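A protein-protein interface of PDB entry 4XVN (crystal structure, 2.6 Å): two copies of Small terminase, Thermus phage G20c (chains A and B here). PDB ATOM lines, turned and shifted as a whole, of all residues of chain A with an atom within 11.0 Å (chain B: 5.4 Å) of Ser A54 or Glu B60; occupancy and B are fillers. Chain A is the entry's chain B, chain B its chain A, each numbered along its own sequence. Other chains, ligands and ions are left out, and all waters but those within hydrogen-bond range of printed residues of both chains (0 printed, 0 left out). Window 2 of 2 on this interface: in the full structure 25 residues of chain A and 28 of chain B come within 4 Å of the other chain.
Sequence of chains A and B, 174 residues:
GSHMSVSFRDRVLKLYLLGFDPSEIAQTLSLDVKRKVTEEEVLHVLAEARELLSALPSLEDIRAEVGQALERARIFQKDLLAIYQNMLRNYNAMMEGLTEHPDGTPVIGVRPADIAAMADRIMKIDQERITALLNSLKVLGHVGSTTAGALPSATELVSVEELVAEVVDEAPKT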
ATOM      1  N   LEU A  13       3.264  -7.251 -32.434  1.00  0.00           N
ATOM      2  CA  LEU A  13       3.149  -6.187 -31.433  1.00  0.00           C
ATOM      3  C   LEU A  13       4.316  -6.196 -30.440  1.00  0.00           C
ATOM      4  O   LEU A  13       4.736  -5.137 -29.974  1.00  0.00           O
ATOM      5  CB  LEU A  13       1.818  -6.307 -30.679  1.00  0.00           C
ATOM      6  CG  LEU A  13       1.498  -5.279 -29.587  1.00  0.00           C
ATOM      7  CD1 LEU A  13       1.587  -3.852 -30.111  1.00  0.00           C
ATOM      8  CD2 LEU A  13       0.117  -5.554 -29.010  1.00  0.00           C
ATOM      9  N   VAL A  45      -1.555  -4.494 -39.246  1.00  0.00           N
ATOM     10  CA  VAL A  45      -1.748  -5.283 -38.018  1.00  0.00           C
ATOM     11  C   VAL A  45      -1.478  -4.427 -36.771  1.00  0.00           C
ATOM     12  O   VAL A  45      -2.185  -4.552 -35.768  1.00  0.00           O
ATOM     13  CB  VAL A  45      -0.864  -6.563 -38.011  1.00  0.00           C
ATOM     14  CG1 VAL A  45      -0.932  -7.291 -36.669  1.00  0.00           C
ATOM     15  CG2 VAL A  45      -1.283  -7.510 -39.130  1.00  0.00           C
ATOM     16  N   LEU A  46      -0.463  -3.565 -36.847  1.00  0.00           N
ATOM     17  CA  LEU A  46      -0.157  -2.613 -35.772  1.00  0.00           C
ATOM     18  C   LEU A  46      -1.252  -1.552 -35.609  1.00  0.00           C
ATOM     19  O   LEU A  46      -1.552  -1.142 -34.487  1.00  0.00           O
ATOM     20  CB  LEU A  46       1.193  -1.928 -36.016  1.00  0.00           C
ATOM     21  CG  LEU A  46       2.437  -2.825 -36.010  1.00  0.00           C
ATOM     22  CD1 LEU A  46       3.646  -2.061 -36.532  1.00  0.00           C
ATOM     23  CD2 LEU A  46       2.713  -3.382 -34.622  1.00  0.00           C
ATOM     24  N   ALA A  47      -1.831  -1.111 -36.727  1.00  0.00           N
ATOM     25  CA  ALA A  47      -2.953  -0.163 -36.714  1.00  0.00           C
ATOM     26  C   ALA A  47      -4.216  -0.765 -36.086  1.00  0.00           C
ATOM     27  O   ALA A  47      -4.936  -0.077 -35.357  1.00  0.00           O
ATOM     28  CB  ALA A  47      -3.249   0.331 -38.123  1.00  0.00           C
ATOM     29  N   GLU A  48      -4.479  -2.039 -36.377  1.00  0.00           N
ATOM     30  CA  GLU A  48      -5.567  -2.784 -35.730  1.00  0.00           C
ATOM     31  C   GLU A  48      -5.279  -3.044 -34.248  1.00  0.00           C
ATOM     32  O   GLU A  48      -6.183  -2.953 -33.415  1.00  0.00           O
ATOM     33  CB  GLU A  48      -5.833  -4.109 -36.454  1.00  0.00           C
ATOM     34  CG  GLU A  48      -6.486  -3.942 -37.818  1.00  0.00           C
ATOM     35  CD  GLU A  48      -6.772  -5.265 -38.506  1.00  0.00           C
ATOM     36  OE1 GLU A  48      -5.869  -6.127 -38.551  1.00  0.00           O
ATOM     37  OE2 GLU A  48      -7.900  -5.440 -39.016  1.00  0.00           O
ATOM     38  N   ALA A  49      -4.025  -3.371 -33.932  1.00  0.00           N
ATOM     39  CA  ALA A  49      -3.578  -3.550 -32.542  1.00  0.00           C
ATOM     40  C   ALA A  49      -3.645  -2.260 -31.716  1.00  0.00           C
ATOM     41  O   ALA A  49      -3.815  -2.315 -30.497  1.00  0.00           O
ATOM     42  CB  ALA A  49      -2.165  -4.115 -32.509  1.00  0.00           C
ATOM     43  N   ARG A  50      -3.500  -1.113 -32.382  1.00  0.00           N
ATOM     44  CA  ARG A  50      -3.618   0.203 -31.741  1.00  0.00           C
ATOM     45  C   ARG A  50      -5.019   0.435 -31.167  1.00  0.00           C
ATOM     46  O   ARG A  50      -5.157   0.896 -30.033  1.00  0.00           O
ATOM     47  CB  ARG A  50      -3.273   1.319 -32.739  1.00  0.00           C
ATOM     48  CG  ARG A  50      -2.945   2.663 -32.109  1.00  0.00           C
ATOM     49  CD  ARG A  50      -2.694   3.723 -33.174  1.00  0.00           C
ATOM     50  NE  ARG A  50      -1.844   4.813 -32.692  1.00  0.00           N
ATOM     51  CZ  ARG A  50      -0.517   4.756 -32.546  1.00  0.00           C
ATOM     52  NH1 ARG A  50       0.171   3.649 -32.835  1.00  0.00           N
ATOM     53  NH2 ARG A  50       0.138   5.825 -32.097  1.00  0.00           N
ATOM     54  N   GLU A  51      -6.045   0.113 -31.956  1.00  0.00           N
ATOM     55  CA  GLU A  51      -7.446   0.246 -31.527  1.00  0.00           C
ATOM     56  C   GLU A  51      -7.817  -0.688 -30.368  1.00  0.00           C
ATOM     57  O   GLU A  51      -8.636  -0.323 -29.523  1.00  0.00           O
ATOM     58  CB  GLU A  51      -8.403   0.008 -32.702  1.00  0.00           C
ATOM     59  CG  GLU A  51      -8.357   1.088 -33.772  1.00  0.00           C
ATOM     60  CD  GLU A  51      -9.447   0.924 -34.816  1.00  0.00           C
ATOM     61  OE1 GLU A  51      -9.623  -0.202 -35.327  1.00  0.00           O
ATOM     62  OE2 GLU A  51     -10.127   1.925 -35.132  1.00  0.00           O
ATOM     63  N   LEU A  52      -7.222  -1.881 -30.339  1.00  0.00           N
ATOM     64  CA  LEU A  52      -7.422  -2.831 -29.235  1.00  0.00           C
ATOM     65  C   LEU A  52      -6.848  -2.287 -27.926  1.00  0.00           C
ATOM     66  O   LEU A  52      -7.513  -2.324 -26.889  1.00  0.00           O
ATOM     67  CB  LEU A  52      -6.784  -4.189 -29.558  1.00  0.00           C
ATOM     68  CG  LEU A  52      -7.380  -4.976 -30.730  1.00  0.00           C
ATOM     69  CD1 LEU A  52      -6.503  -6.171 -31.078  1.00  0.00           C
ATOM     70  CD2 LEU A  52      -8.801  -5.429 -30.423  1.00  0.00           C
ATOM     71  N   LEU A  53      -5.615  -1.784 -27.990  1.00  0.00           N
ATOM     72  CA  LEU A  53      -4.964  -1.135 -26.844  1.00  0.00           C
ATOM     73  C   LEU A  53      -5.616   0.201 -26.464  1.00  0.00           C
ATOM     74  O   LEU A  53      -5.584   0.593 -25.295  1.00  0.00           O
ATOM     75  CB  LEU A  53      -3.471  -0.923 -27.127  1.00  0.00           C
ATOM     76  CG  LEU A  53      -2.619  -2.186 -27.296  1.00  0.00           C
ATOM     77  CD1 LEU A  53      -1.248  -1.834 -27.854  1.00  0.00           C
ATOM     78  CD2 LEU A  53      -2.486  -2.946 -25.983  1.00  0.00           C
ATOM     79  N   SER A  54      -6.194   0.893 -27.447  1.00  0.00           N
ATOM     80  CA  SER A  54      -6.930   2.145 -27.206  1.00  0.00           C
ATOM     81  C   SER A  54      -8.252   1.978 -26.440  1.00  0.00           C
ATOM     82  O   SER A  54      -8.783   2.962 -25.925  1.00  0.00           O
ATOM     83  CB  SER A  54      -7.217   2.860 -28.531  1.00  0.00           C
ATOM     84  OG  SER A  54      -6.016   3.218 -29.187  1.00  0.00           O
ATOM     85  N   ALA A  55      -8.788   0.757 -26.386  1.00  0.00           N
ATOM     86  CA  ALA A  55     -10.038   0.482 -25.668  1.00  0.00           C
ATOM     87  C   ALA A  55      -9.882   0.692 -24.160  1.00  0.00           C
ATOM     88  O   ALA A  55      -8.871   0.296 -23.576  1.00  0.00           O
ATOM     89  CB  ALA A  55     -10.513  -0.935 -25.954  1.00  0.00           C
ATOM     90  N   LEU A  56     -10.888   1.315 -23.547  1.00  0.00           N
ATOM     91  CA  LEU A  56     -10.885   1.589 -22.108  1.00  0.00           C
ATOM     92  C   LEU A  56     -11.096   0.284 -21.332  1.00  0.00           C
ATOM     93  O   LEU A  56     -11.981  -0.499 -21.685  1.00  0.00           O
ATOM     94  CB  LEU A  56     -11.990   2.589 -21.753  1.00  0.00           C
ATOM     95  CG  LEU A  56     -12.024   3.158 -20.327  1.00  0.00           C
ATOM     96  CD1 LEU A  56     -10.929   4.196 -20.120  1.00  0.00           C
ATOM     97  CD2 LEU A  56     -13.388   3.765 -20.028  1.00  0.00           C
ATOM     98  N   PRO A  57     -10.291   0.045 -20.276  1.00  0.00           N
ATOM     99  CA  PRO A  57     -10.432  -1.192 -19.507  1.00  0.00           C
ATOM    100  C   PRO A  57     -11.633  -1.163 -18.559  1.00  0.00           C
ATOM    101  O   PRO A  57     -11.988  -0.103 -18.036  1.00  0.00           O
ATOM    102  CB  PRO A  57      -9.125  -1.255 -18.716  1.00  0.00           C
ATOM    103  CG  PRO A  57      -8.772   0.172 -18.493  1.00  0.00           C
ATOM    104  CD  PRO A  57      -9.232   0.911 -19.718  1.00  0.00           C
ATOM    105  N   SER A  58     -12.239  -2.328 -18.344  1.00  0.00           N
ATOM    106  CA  SER A  58     -13.364  -2.468 -17.419  1.00  0.00           C
ATOM    107  C   SER A  58     -12.874  -2.471 -15.971  1.00  0.00           C
ATOM    108  O   SER A  58     -11.670  -2.541 -15.714  1.00  0.00           O
ATOM    109  CB  SER A  58     -14.132  -3.763 -17.702  1.00  0.00           C
ATOM    110  OG  SER A  58     -14.429  -3.892 -19.081  1.00  0.00           O
ATOM    111  N   SER B  58      -6.064  13.585 -29.270  1.00  0.00           N
ATOM    112  CA  SER B  58      -7.414  13.104 -28.961  1.00  0.00           C
ATOM    113  C   SER B  58      -7.406  12.312 -27.652  1.00  0.00           C
ATOM    114  O   SER B  58      -6.343  11.941 -27.147  1.00  0.00           O
ATOM    115  CB  SER B  58      -7.952  12.232 -30.099  1.00  0.00           C
ATOM    116  OG  SER B  58      -9.301  11.861 -29.870  1.00  0.00           O
ATOM    117  N   LEU B  59      -8.596  12.054 -27.114  1.00  0.00           N
ATOM    118  CA  LEU B  59      -8.735  11.301 -25.860  1.00  0.00           C
ATOM    119  C   LEU B  59      -8.420   9.810 -26.031  1.00  0.00           C
ATOM    120  O   LEU B  59      -7.887   9.187 -25.110  1.00  0.00           O
ATOM    121  CB  LEU B  59     -10.135  11.493 -25.256  1.00  0.00           C
ATOM    122  CG  LEU B  59     -10.479  12.917 -24.794  1.00  0.00           C
ATOM    123  CD1 LEU B  59     -11.940  13.015 -24.384  1.00  0.00           C
ATOM    124  CD2 LEU B  59      -9.579  13.371 -23.652  1.00  0.00           C
ATOM    125  N   GLU B  60      -8.745   9.245 -27.195  1.00  0.00           N
ATOM    126  CA  GLU B  60      -8.359   7.864 -27.528  1.00  0.00           C
ATOM    127  C   GLU B  60      -6.885   7.736 -27.946  1.00  0.00           C
ATOM    128  O   GLU B  60      -6.301   6.658 -27.811  1.00  0.00           O
ATOM    129  CB  GLU B  60      -9.271   7.280 -28.613  1.00  0.00           C
ATOM    130  CG  GLU B  60     -10.706   7.060 -28.151  1.00  0.00           C
ATOM    131  CD  GLU B  60     -11.515   6.175 -29.086  1.00  0.00           C
ATOM    132  OE1 GLU B  60     -11.155   6.053 -30.278  1.00  0.00           O
ATOM    133  OE2 GLU B  60     -12.524   5.600 -28.626  1.00  0.00           O
ATOM    134  N   ASP B  61      -6.297   8.819 -28.459  1.00  0.00           N
ATOM    135  CA  ASP B  61      -4.851   8.869 -28.736  1.00  0.00           C
ATOM    136  C   ASP B  61      -4.013   8.798 -27.454  1.00  0.00           C
ATOM    137  O   ASP B  61      -2.899   8.273 -27.475  1.00  0.00           O
ATOM    138  CB  ASP B  61      -4.478  10.128 -29.534  1.00  0.00           C
ATOM    139  CG  ASP B  61      -5.018  10.110 -30.960  1.00  0.00           C
ATOM    140  OD1 ASP B  61      -5.842   9.229 -31.296  1.00  0.00           O
ATOM    141  OD2 ASP B  61      -4.618  10.993 -31.750  1.00  0.00           O
ATOM    142  N   ILE B  62      -4.549   9.328 -26.353  1.00  0.00           N
ATOM    143  CA  ILE B  62      -3.941   9.166 -25.024  1.00  0.00           C
ATOM    144  C   ILE B  62      -4.036   7.699 -24.593  1.00  0.00           C
ATOM    145  O   ILE B  62      -3.056   7.129 -24.115  1.00  0.00           O
ATOM    146  CB  ILE B  62      -4.607  10.080 -23.961  1.00  0.00           C
ATOM    147  CG1 ILE B  62      -4.360  11.560 -24.294  1.00  0.00           C
ATOM    148  CG2 ILE B  62      -4.074   9.778 -22.558  1.00  0.00           C
ATOM    149  CD1 ILE B  62      -5.322  12.517 -23.621  1.00  0.00           C
ATOM    150  N   ARG B  63      -5.216   7.101 -24.771  1.00  0.00           N
ATOM    151  CA  ARG B  63      -5.434   5.678 -24.476  1.00  0.00           C
ATOM    152  C   ARG B  63      -4.580   4.754 -25.351  1.00  0.00           C
ATOM    153  O   ARG B  63      -4.182   3.676 -24.907  1.00  0.00           O
ATOM    154  CB  ARG B  63      -6.911   5.303 -24.646  1.00  0.00           C
ATOM    155  CG  ARG B  63      -7.859   5.952 -23.651  1.00  0.00           C
ATOM    156  CD  ARG B  63      -9.303   5.655 -24.021  1.00  0.00           C
ATOM    157  NE  ARG B  63     -10.260   6.275 -23.104  1.00  0.00           N
ATOM    158  CZ  ARG B  63     -11.588   6.186 -23.207  1.00  0.00           C
ATOM    159  NH1 ARG B  63     -12.156   5.498 -24.198  1.00  0.00           N
ATOM    160  NH2 ARG B  63     -12.359   6.793 -22.308  1.00  0.00           N
ATOM    161  N   ALA B  64      -4.320   5.175 -26.591  1.00  0.00           N
ATOM    162  CA  ALA B  64      -3.430   4.448 -27.504  1.00  0.00           C
ATOM    163  C   ALA B  64      -2.005   4.371 -26.958  1.00  0.00           C
ATOM    164  O   ALA B  64      -1.393   3.303 -26.964  1.00  0.00           O
ATOM    165  CB  ALA B  64      -3.426   5.099 -28.881  1.00  0.00           C
ATOM    166  N   GLU B  65      -1.490   5.506 -26.489  1.00  0.00           N
ATOM    167  CA  GLU B  65      -0.152   5.574 -25.890  1.00  0.00           C
ATOM    168  C   GLU B  65      -0.083   4.877 -24.528  1.00  0.00           C
ATOM    169  O   GLU B  65       0.920   4.231 -24.218  1.00  0.00           O
ATOM    170  CB  GLU B  65       0.312   7.032 -25.753  1.00  0.00           C
ATOM    171  CG  GLU B  65       0.521   7.761 -27.079  1.00  0.00           C
ATOM    172  CD  GLU B  65       1.653   7.195 -27.927  1.00  0.00           C
ATOM    173  OE1 GLU B  65       2.564   6.537 -27.378  1.00  0.00           O
ATOM    174  OE2 GLU B  65       1.635   7.415 -29.156  1.00  0.00           O
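The backbone carbonyl oxygen (O) of Leu A53 sits close to the backbone carbonyl oxygen (O) of Arg B63 (3.4 Å). The guanidinium group (NH2) of Arg A50 is in salt-bridge range of the side-chain carboxylate (OE2) of Glu B65 (3.7 Å).
The side-chain hydroxyl (OG) of Ser A54 sits at hydrogen-bond distance from the backbone carbonyl oxygen (O) of Arg A50 (2.6 Å).
OG of Ser A54 touches O of Glu B60, at 3.7 Å. Arg B63 touches Ser A54 (CB to O, 3.3 Å). Ser A54 touches Ala B64. Leu A56 touches Arg B63.
Printed residues of chain B within 4 Å of Ser A54: Glu B60 (3.7 Å), Arg B63 (3.3 Å) and Ala B64 (3.2 Å). Of chain A, only Ser A54 comes within 4 Å of Glu B60. No residue of chain A comes within 4 Å of Ser B58. No residue of chain A comes within 4 Å of Leu B59. No residue of chain A comes within 4 Å of Asp B61. Ile B62 touches none of the printed residues of chain A. Of chain A, only Leu A53 (3.4 Å), Ser A54 (3.3 Å) and Leu A56 (3.7 Å) come within 4 Å of Arg B63. Printed residues of chain B within 4 Å of Arg A50: Glu B65. Printed residues of chain A within 4 Å of Glu B65: Arg A50 (3.7 Å). Ser A58 touches none of the printed residues of chain B.
Of the 8 printed residues of chain B, 4 touch a printed residue of chain A. Hydrophobic or aromatic side chains of chain B within 4 Å of the printed part of chain A: Ala B64. Along chain B the printed residues that touch a printed residue of chain A span positions 60 to 65. Among the printed residues, 6 pairs touch across the chains. Among the printed residues, Asp or Glu carboxylates within 4 Å of a Lys or Arg side-chain nitrogen of the other chain: Arg A50 with Glu B65.
Position printed for both chains: 58.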
